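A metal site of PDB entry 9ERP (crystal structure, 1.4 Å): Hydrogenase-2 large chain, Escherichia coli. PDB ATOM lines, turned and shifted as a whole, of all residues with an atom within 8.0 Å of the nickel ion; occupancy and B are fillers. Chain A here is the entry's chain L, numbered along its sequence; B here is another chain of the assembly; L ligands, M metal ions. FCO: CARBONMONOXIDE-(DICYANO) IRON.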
ATOM      1  N   GLU A  14     -15.790 -15.769  -0.957  1.00  0.00           N
ATOM      2  CA  GLU A  14     -16.660 -14.658  -0.568  1.00  0.00           C
ATOM      3  C   GLU A  14     -16.830 -14.675   0.936  1.00  0.00           C
ATOM      4  O   GLU A  14     -17.228 -15.708   1.509  1.00  0.00           O
ATOM      5  CB  GLU A  14     -18.023 -14.744  -1.256  1.00  0.00           C
ATOM      6  CG  GLU A  14     -18.951 -13.519  -1.043  1.00  0.00           C
ATOM      7  CD  GLU A  14     -19.317 -13.235   0.392  1.00  0.00           C
ATOM      8  OE1 GLU A  14     -19.519 -14.184   1.169  1.00  0.00           O
ATOM      9  OE2 GLU A  14     -19.396 -12.037   0.798  1.00  0.00           O
ATOM     10  N   GLY A  15     -16.560 -13.563   1.578  1.00  0.00           N
ATOM     11  CA  GLY A  15     -16.946 -13.401   2.956  1.00  0.00           C
ATOM     12  C   GLY A  15     -15.870 -13.852   3.930  1.00  0.00           C
ATOM     13  O   GLY A  15     -14.679 -14.001   3.628  1.00  0.00           O
ATOM     14  N   GLN A  58     -31.695 -10.083  -2.007  1.00  0.00           N
ATOM     15  CA  GLN A  58     -30.652 -10.223  -3.013  1.00  0.00           C
ATOM     16  C   GLN A  58     -29.302  -9.833  -2.419  1.00  0.00           C
ATOM     17  O   GLN A  58     -28.252 -10.371  -2.798  1.00  0.00           O
ATOM     18  CB  GLN A  58     -30.923  -9.318  -4.234  1.00  0.00           C
ATOM     19  CG  GLN A  58     -29.920  -9.631  -5.336  1.00  0.00           C
ATOM     20  CD  GLN A  58     -30.227  -9.063  -6.710  1.00  0.00           C
ATOM     21  OE1 GLN A  58     -29.695  -9.531  -7.711  1.00  0.00           O
ATOM     22  NE2 GLN A  58     -30.990  -7.978  -6.749  1.00  0.00           N
ATOM     23  N   ILE A  60     -28.080 -10.578   0.303  1.00  0.00           N
ATOM     24  CA  ILE A  60     -27.346 -11.629   1.003  1.00  0.00           C
ATOM     25  C   ILE A  60     -25.978 -11.810   0.373  1.00  0.00           C
ATOM     26  O   ILE A  60     -24.976 -12.042   1.069  1.00  0.00           O
ATOM     27  CB  ILE A  60     -28.156 -12.944   1.010  1.00  0.00           C
ATOM     28  CG1 ILE A  60     -29.304 -12.822   2.029  1.00  0.00           C
ATOM     29  CG2 ILE A  60     -27.243 -14.119   1.317  1.00  0.00           C
ATOM     30  CD1 ILE A  60     -30.330 -13.959   1.999  1.00  0.00           C
ATOM     31  N   CYS A  61     -25.888 -11.658  -0.953  1.00  0.00           N
ATOM     32  CA  CYS A  61     -24.596 -11.889  -1.598  1.00  0.00           C
ATOM     33  C   CYS A  61     -24.503 -11.188  -2.949  1.00  0.00           C
ATOM     34  O   CYS A  61     -25.435 -11.239  -3.759  1.00  0.00           O
ATOM     35  CB  CYS A  61     -24.384 -13.395  -1.767  1.00  0.00           C
ATOM     36  SG  CYS A  61     -22.763 -13.838  -2.397  1.00  0.00           S
ATOM     37  N   GLY A  62     -23.340 -10.594  -3.190  1.00  0.00           N
ATOM     38  CA  GLY A  62     -23.082  -9.970  -4.471  1.00  0.00           C
ATOM     39  C   GLY A  62     -22.190 -10.759  -5.379  1.00  0.00           C
ATOM     40  O   GLY A  62     -22.013 -10.379  -6.544  1.00  0.00           O
ATOM     41  N   VAL A  63     -21.576 -11.843  -4.868  1.00  0.00           N
ATOM     42  CA  VAL A  63     -20.908 -12.790  -5.760  1.00  0.00           C
ATOM     43  C   VAL A  63     -21.960 -13.612  -6.484  1.00  0.00           C
ATOM     44  O   VAL A  63     -22.096 -13.524  -7.705  1.00  0.00           O
ATOM     45  CB  VAL A  63     -19.950 -13.701  -4.984  1.00  0.00           C
ATOM     46  CG1 VAL A  63     -19.386 -14.760  -5.925  1.00  0.00           C
ATOM     47  CG2 VAL A  63     -18.813 -12.899  -4.364  1.00  0.00           C
ATOM     48  N   CYS A  64     -22.789 -14.332  -5.732  1.00  0.00           N
ATOM     49  CA  CYS A  64     -23.957 -14.983  -6.302  1.00  0.00           C
ATOM     50  C   CYS A  64     -25.128 -14.012  -6.354  1.00  0.00           C
ATOM     51  O   CYS A  64     -26.247 -14.310  -5.902  1.00  0.00           O
ATOM     52  CB  CYS A  64     -24.287 -16.296  -5.589  1.00  0.00           C
ATOM     53  SG  CYS A  64     -24.785 -16.151  -3.865  1.00  0.00           S
ATOM     54  N   THR A  65     -24.888 -12.827  -6.886  1.00  0.00           N
ATOM     55  CA  THR A  65     -25.980 -11.935  -7.213  1.00  0.00           C
ATOM     56  C   THR A  65     -26.942 -12.662  -8.148  1.00  0.00           C
ATOM     57  O   THR A  65     -26.626 -13.683  -8.745  1.00  0.00           O
ATOM     58  CB  THR A  65     -25.438 -10.610  -7.738  1.00  0.00           C
ATOM     59  OG1 THR A  65     -26.496  -9.657  -7.813  1.00  0.00           O
ATOM     60  CG2 THR A  65     -24.813 -10.739  -9.111  1.00  0.00           C
ATOM     61  N   THR A  67     -29.189 -14.706  -7.481  1.00  0.00           N
ATOM     62  CA  THR A  67     -29.724 -15.978  -7.006  1.00  0.00           C
ATOM     63  C   THR A  67     -30.767 -15.806  -5.914  1.00  0.00           C
ATOM     64  O   THR A  67     -31.808 -16.471  -5.932  1.00  0.00           O
ATOM     65  CB  THR A  67     -28.610 -16.936  -6.545  1.00  0.00           C
ATOM     66  OG1 THR A  67     -27.955 -16.435  -5.389  1.00  0.00           O
ATOM     67  CG2 THR A  67     -27.628 -17.241  -7.676  1.00  0.00           C
ATOM     68  N   HIS A  68     -30.471 -14.985  -4.909  1.00  0.00           N
ATOM     69  CA  HIS A  68     -31.430 -14.794  -3.819  1.00  0.00           C
ATOM     70  C   HIS A  68     -32.633 -13.994  -4.276  1.00  0.00           C
ATOM     71  O   HIS A  68     -33.747 -14.155  -3.736  1.00  0.00           O
ATOM     72  CB  HIS A  68     -30.736 -14.120  -2.624  1.00  0.00           C
ATOM     73  CG  HIS A  68     -29.688 -14.972  -2.022  1.00  0.00           C
ATOM     74  ND1 HIS A  68     -29.986 -16.038  -1.183  1.00  0.00           N
ATOM     75  CD2 HIS A  68     -28.336 -14.986  -2.169  1.00  0.00           C
ATOM     76  CE1 HIS A  68     -28.872 -16.636  -0.830  1.00  0.00           C
ATOM     77  NE2 HIS A  68     -27.858 -16.016  -1.398  1.00  0.00           N
ATOM     78  N   HIS A  99     -25.207 -15.301 -15.426  1.00  0.00           N
ATOM     79  CA  HIS A  99     -24.555 -15.015 -14.162  1.00  0.00           C
ATOM     80  C   HIS A  99     -23.657 -16.161 -13.734  1.00  0.00           C
ATOM     81  O   HIS A  99     -22.508 -15.966 -13.305  1.00  0.00           O
ATOM     82  CB  HIS A  99     -25.557 -14.768 -13.028  1.00  0.00           C
ATOM     83  CG  HIS A  99     -24.830 -14.750 -11.719  1.00  0.00           C
ATOM     84  ND1 HIS A  99     -24.101 -13.653 -11.308  1.00  0.00           N
ATOM     85  CD2 HIS A  99     -24.536 -15.751 -10.861  1.00  0.00           C
ATOM     86  CE1 HIS A  99     -23.437 -13.966 -10.218  1.00  0.00           C
ATOM     87  NE2 HIS A  99     -23.690 -15.234  -9.916  1.00  0.00           N
ATOM     88  N   ASP A 103     -19.741 -16.486 -12.718  1.00  0.00           N
ATOM     89  CA  ASP A 103     -19.408 -16.911 -11.367  1.00  0.00           C
ATOM     90  C   ASP A 103     -18.396 -18.065 -11.414  1.00  0.00           C
ATOM     91  O   ASP A 103     -17.309 -17.987 -10.821  1.00  0.00           O
ATOM     92  CB  ASP A 103     -20.731 -17.287 -10.681  1.00  0.00           C
ATOM     93  CG  ASP A 103     -20.682 -17.260  -9.177  1.00  0.00           C
ATOM     94  OD1 ASP A 103     -19.637 -17.574  -8.595  1.00  0.00           O
ATOM     95  OD2 ASP A 103     -21.755 -16.990  -8.580  1.00  0.00           O
ATOM     96  N   ALA A 477     -28.343 -22.934  -7.575  1.00  0.00           N
ATOM     97  CA  ALA A 477     -27.423 -21.798  -7.648  1.00  0.00           C
ATOM     98  C   ALA A 477     -26.042 -22.287  -8.004  1.00  0.00           C
ATOM     99  O   ALA A 477     -25.765 -23.495  -8.006  1.00  0.00           O
ATOM    100  CB  ALA A 477     -27.387 -21.103  -6.297  1.00  0.00           C
ATOM    101  N   PRO A 478     -25.118 -21.369  -8.325  1.00  0.00           N
ATOM    102  CA  PRO A 478     -23.752 -21.796  -8.646  1.00  0.00           C
ATOM    103  C   PRO A 478     -23.120 -22.708  -7.615  1.00  0.00           C
ATOM    104  O   PRO A 478     -22.354 -23.597  -7.971  1.00  0.00           O
ATOM    105  CB  PRO A 478     -22.999 -20.470  -8.760  1.00  0.00           C
ATOM    106  CG  PRO A 478     -24.050 -19.457  -9.215  1.00  0.00           C
ATOM    107  CD  PRO A 478     -25.308 -19.909  -8.492  1.00  0.00           C
ATOM    108  N   ARG A 479     -23.449 -22.533  -6.346  1.00  0.00           N
ATOM    109  CA  ARG A 479     -22.870 -23.307  -5.261  1.00  0.00           C
ATOM    110  C   ARG A 479     -23.790 -24.404  -4.765  1.00  0.00           C
ATOM    111  O   ARG A 479     -23.402 -25.147  -3.843  1.00  0.00           O
ATOM    112  CB  ARG A 479     -22.442 -22.384  -4.130  1.00  0.00           C
ATOM    113  CG  ARG A 479     -21.277 -21.501  -4.553  1.00  0.00           C
ATOM    114  CD  ARG A 479     -21.081 -20.276  -3.710  1.00  0.00           C
ATOM    115  NE  ARG A 479     -20.014 -19.447  -4.243  1.00  0.00           N
ATOM    116  CZ  ARG A 479     -20.155 -18.695  -5.333  1.00  0.00           C
ATOM    117  NH1 ARG A 479     -21.347 -18.478  -5.876  1.00  0.00           N
ATOM    118  NH2 ARG A 479     -19.097 -18.135  -5.878  1.00  0.00           N
ATOM    119  N   VAL A 500     -29.101 -21.908   2.447  1.00  0.00           N
ATOM    120  CA  VAL A 500     -28.295 -21.499   1.293  1.00  0.00           C
ATOM    121  C   VAL A 500     -27.291 -22.613   1.015  1.00  0.00           C
ATOM    122  O   VAL A 500     -26.903 -23.326   1.941  1.00  0.00           O
ATOM    123  CB  VAL A 500     -27.669 -20.131   1.592  1.00  0.00           C
ATOM    124  CG1 VAL A 500     -26.965 -19.552   0.420  1.00  0.00           C
ATOM    125  CG2 VAL A 500     -28.755 -19.173   2.059  1.00  0.00           C
ATOM    126  N   PRO A 501     -26.834 -22.813  -0.236  1.00  0.00           N
ATOM    127  CA  PRO A 501     -25.957 -23.971  -0.468  1.00  0.00           C
ATOM    128  C   PRO A 501     -24.712 -24.005   0.417  1.00  0.00           C
ATOM    129  O   PRO A 501     -24.359 -25.075   0.938  1.00  0.00           O
ATOM    130  CB  PRO A 501     -25.660 -23.929  -1.982  1.00  0.00           C
ATOM    131  CG  PRO A 501     -26.130 -22.582  -2.451  1.00  0.00           C
ATOM    132  CD  PRO A 501     -27.276 -22.208  -1.520  1.00  0.00           C
ATOM    133  N   SER A 502     -24.061 -22.868   0.622  1.00  0.00           N
ATOM    134  CA  SER A 502     -22.879 -22.899   1.486  1.00  0.00           C
ATOM    135  C   SER A 502     -23.250 -23.176   2.940  1.00  0.00           C
ATOM    136  O   SER A 502     -22.372 -23.590   3.696  1.00  0.00           O
ATOM    137  CB  SER A 502     -22.062 -21.616   1.348  1.00  0.00           C
ATOM    138  OG  SER A 502     -21.440 -21.549   0.062  1.00  0.00           O
ATOM    139  N   ASP A 544     -16.166 -23.701  -3.303  1.00  0.00           N
ATOM    140  CA  ASP A 544     -16.545 -22.319  -3.672  1.00  0.00           C
ATOM    141  C   ASP A 544     -17.300 -21.676  -2.514  1.00  0.00           C
ATOM    142  O   ASP A 544     -18.460 -21.249  -2.665  1.00  0.00           O
ATOM    143  CB  ASP A 544     -17.349 -22.402  -4.970  1.00  0.00           C
ATOM    144  CG  ASP A 544     -17.678 -21.051  -5.586  1.00  0.00           C
ATOM    145  OD1 ASP A 544     -17.138 -20.033  -5.172  1.00  0.00           O
ATOM    146  OD2 ASP A 544     -18.469 -21.092  -6.553  1.00  0.00           O
ATOM    147  N   PRO A 545     -16.645 -21.524  -1.359  1.00  0.00           N
ATOM    148  CA  PRO A 545     -17.349 -20.972  -0.195  1.00  0.00           C
ATOM    149  C   PRO A 545     -17.870 -19.564  -0.412  1.00  0.00           C
ATOM    150  O   PRO A 545     -17.172 -18.689  -0.926  1.00  0.00           O
ATOM    151  CB  PRO A 545     -16.295 -20.997   0.914  1.00  0.00           C
ATOM    152  CG  PRO A 545     -15.342 -22.053   0.486  1.00  0.00           C
ATOM    153  CD  PRO A 545     -15.273 -21.926  -1.013  1.00  0.00           C
ATOM    154  N   CYS A 546     -19.091 -19.341   0.046  1.00  0.00           N
ATOM    155  CA  CYS A 546     -19.681 -18.007   0.076  1.00  0.00           C
ATOM    156  C   CYS A 546     -20.265 -17.851   1.487  1.00  0.00           C
ATOM    157  O   CYS A 546     -21.293 -18.439   1.822  1.00  0.00           O
ATOM    158  CB  CYS A 546     -20.737 -17.866  -0.980  1.00  0.00           C
ATOM    159  SG  CYS A 546     -21.328 -16.153  -1.036  1.00  0.00           S
ATOM    160  N   MET A 547     -19.579 -17.099   2.324  1.00  0.00           N
ATOM    161  CA  MET A 547     -19.983 -17.049   3.742  1.00  0.00           C
ATOM    162  C   MET A 547     -21.035 -15.994   4.022  1.00  0.00           C
ATOM    163  O   MET A 547     -21.776 -16.129   5.008  1.00  0.00           O
ATOM    164  CB  MET A 547     -18.764 -16.834   4.630  1.00  0.00           C
ATOM    165  CG  MET A 547     -17.717 -17.973   4.601  1.00  0.00           C
ATOM    166  SD  MET A 547     -18.351 -19.647   4.473  1.00  0.00           S
ATOM    167  CE  MET A 547     -18.884 -19.893   6.140  1.00  0.00           C
ATOM    168  N   ALA A 548     -21.146 -14.965   3.178  1.00  0.00           N
ATOM    169  CA  ALA A 548     -22.315 -14.103   3.236  1.00  0.00           C
ATOM    170  C   ALA A 548     -23.551 -14.929   2.947  1.00  0.00           C
ATOM    171  O   ALA A 548     -24.572 -14.819   3.614  1.00  0.00           O
ATOM    172  CB  ALA A 548     -22.159 -12.939   2.246  1.00  0.00           C
ATOM    173  N   CYS A 549     -23.450 -15.816   1.957  1.00  0.00           N
ATOM    174  CA  CYS A 549     -24.521 -16.768   1.711  1.00  0.00           C
ATOM    175  C   CYS A 549     -24.751 -17.711   2.882  1.00  0.00           C
ATOM    176  O   CYS A 549     -25.892 -17.969   3.276  1.00  0.00           O
ATOM    177  CB  CYS A 549     -24.180 -17.595   0.478  1.00  0.00           C
ATOM    178  SG  CYS A 549     -24.711 -16.794  -1.017  1.00  0.00           S
ATOM    179  N   ALA A 550     -23.666 -18.308   3.408  1.00  0.00           N
ATOM    180  CA  ALA A 550     -23.844 -19.375   4.382  1.00  0.00           C
ATOM    181  C   ALA A 550     -24.547 -18.850   5.622  1.00  0.00           C
ATOM    182  O   ALA A 550     -25.348 -19.563   6.218  1.00  0.00           O
ATOM    183  CB  ALA A 550     -22.483 -19.958   4.788  1.00  0.00           C
ATOM    184  N   CYS B  21     -21.398  -7.817   1.298  1.00  0.00           N
ATOM    185  CA  CYS B  21     -21.922  -8.928   0.499  1.00  0.00           C
ATOM    186  C   CYS B  21     -21.003  -9.272  -0.665  1.00  0.00           C
ATOM    187  O   CYS B  21     -21.260 -10.269  -1.368  1.00  0.00           O
ATOM    188  CB  CYS B  21     -23.321  -8.596  -0.011  1.00  0.00           C
ATOM    189  SG  CYS B  21     -23.311  -7.576  -1.515  1.00  0.00           S
ATOM    190  N   THR B  22     -19.928  -8.490  -0.868  1.00  0.00           N
ATOM    191  CA  THR B  22     -18.886  -8.608  -1.884  1.00  0.00           C
ATOM    192  C   THR B  22     -19.357  -7.972  -3.197  1.00  0.00           C
ATOM    193  O   THR B  22     -18.560  -7.822  -4.118  1.00  0.00           O
ATOM    194  CB  THR B  22     -18.365 -10.029  -2.019  1.00  0.00           C
ATOM    195  OG1 THR B  22     -18.073 -10.522  -0.694  1.00  0.00           O
ATOM    196  CG2 THR B  22     -17.097 -10.097  -2.826  1.00  0.00           C
HETATM  197 FE   FCO L   1     -24.606 -18.184  -2.860  1.00  0.00          FE
HETATM  198  C1  FCO L   1     -24.043 -19.616  -1.845  1.00  0.00           C
HETATM  199  N1  FCO L   1     -23.652 -20.503  -1.188  1.00  0.00           N
HETATM  200  C2  FCO L   1     -24.327 -19.111  -4.424  1.00  0.00           C
HETATM  201  N2  FCO L   1     -24.152 -19.757  -5.394  1.00  0.00           N
HETATM  202  C3  FCO L   1     -26.308 -18.686  -2.918  1.00  0.00           C
HETATM  203  O3  FCO L   1     -27.383 -19.099  -3.012  1.00  0.00           O
HETATM  204 NI    NI M   1     -22.985 -16.000  -2.378  1.00  0.00          NI
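The side-chain sulfur of Cys 546 lies close to the side-chain carboxylate of Glu 14, at 3.5 Å. N of Cys 546 lies within hydrogen-bond range of OG of Ser 502. The backbone NH (N) of Val 63 sits close to the side-chain sulfur (SG) of Cys 61. A ring nitrogen (NE2) of His 68 lies close to the side-chain sulfur (SG) of Cys 549, at 3.3 Å. The backbone carbonyl oxygen of Cys 64 lies within hydrogen-bond range of the side-chain hydroxyl of Thr 67 (2.8 Å).
Four residues have an atom within 4 Å of the nickel ion: Cys 61, Cys 64, Cys 546 and Cys 549. The nearest printed residue that does not touch the nickel ion is Arg 479 (4.6 Å).
The side-chain sulfur (SG) of Cys 549 binds an iron atom (FE) of the ligand, at 2.3 Å. FE of the ligand is bound by SG of Cys 64 (2.3 Å). A nitrogen (N2) of the ligand is in hydrogen-bond range of the backbone NH of Arg 479 (3.0 Å). A nitrogen (N2) of the ligand is in hydrogen-bond range of the guanidinium group (NH1) of Arg 479 (3.1 Å). The backbone NH (N) of Ser 502 is in hydrogen-bond range of a nitrogen (N1) of the ligand (3.0 Å). OG of Ser 502 is in hydrogen-bond range of N1 of the ligand, at 2.7 Å.
The nickel ion is bound by SG of Cys 546 (2.1 Å), SG of Cys 61 (2.2 Å), SG of Cys 549 (2.3 Å) and SG of Cys 64 (2.3 Å). The nickel ion has four donor atoms within binding distance.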
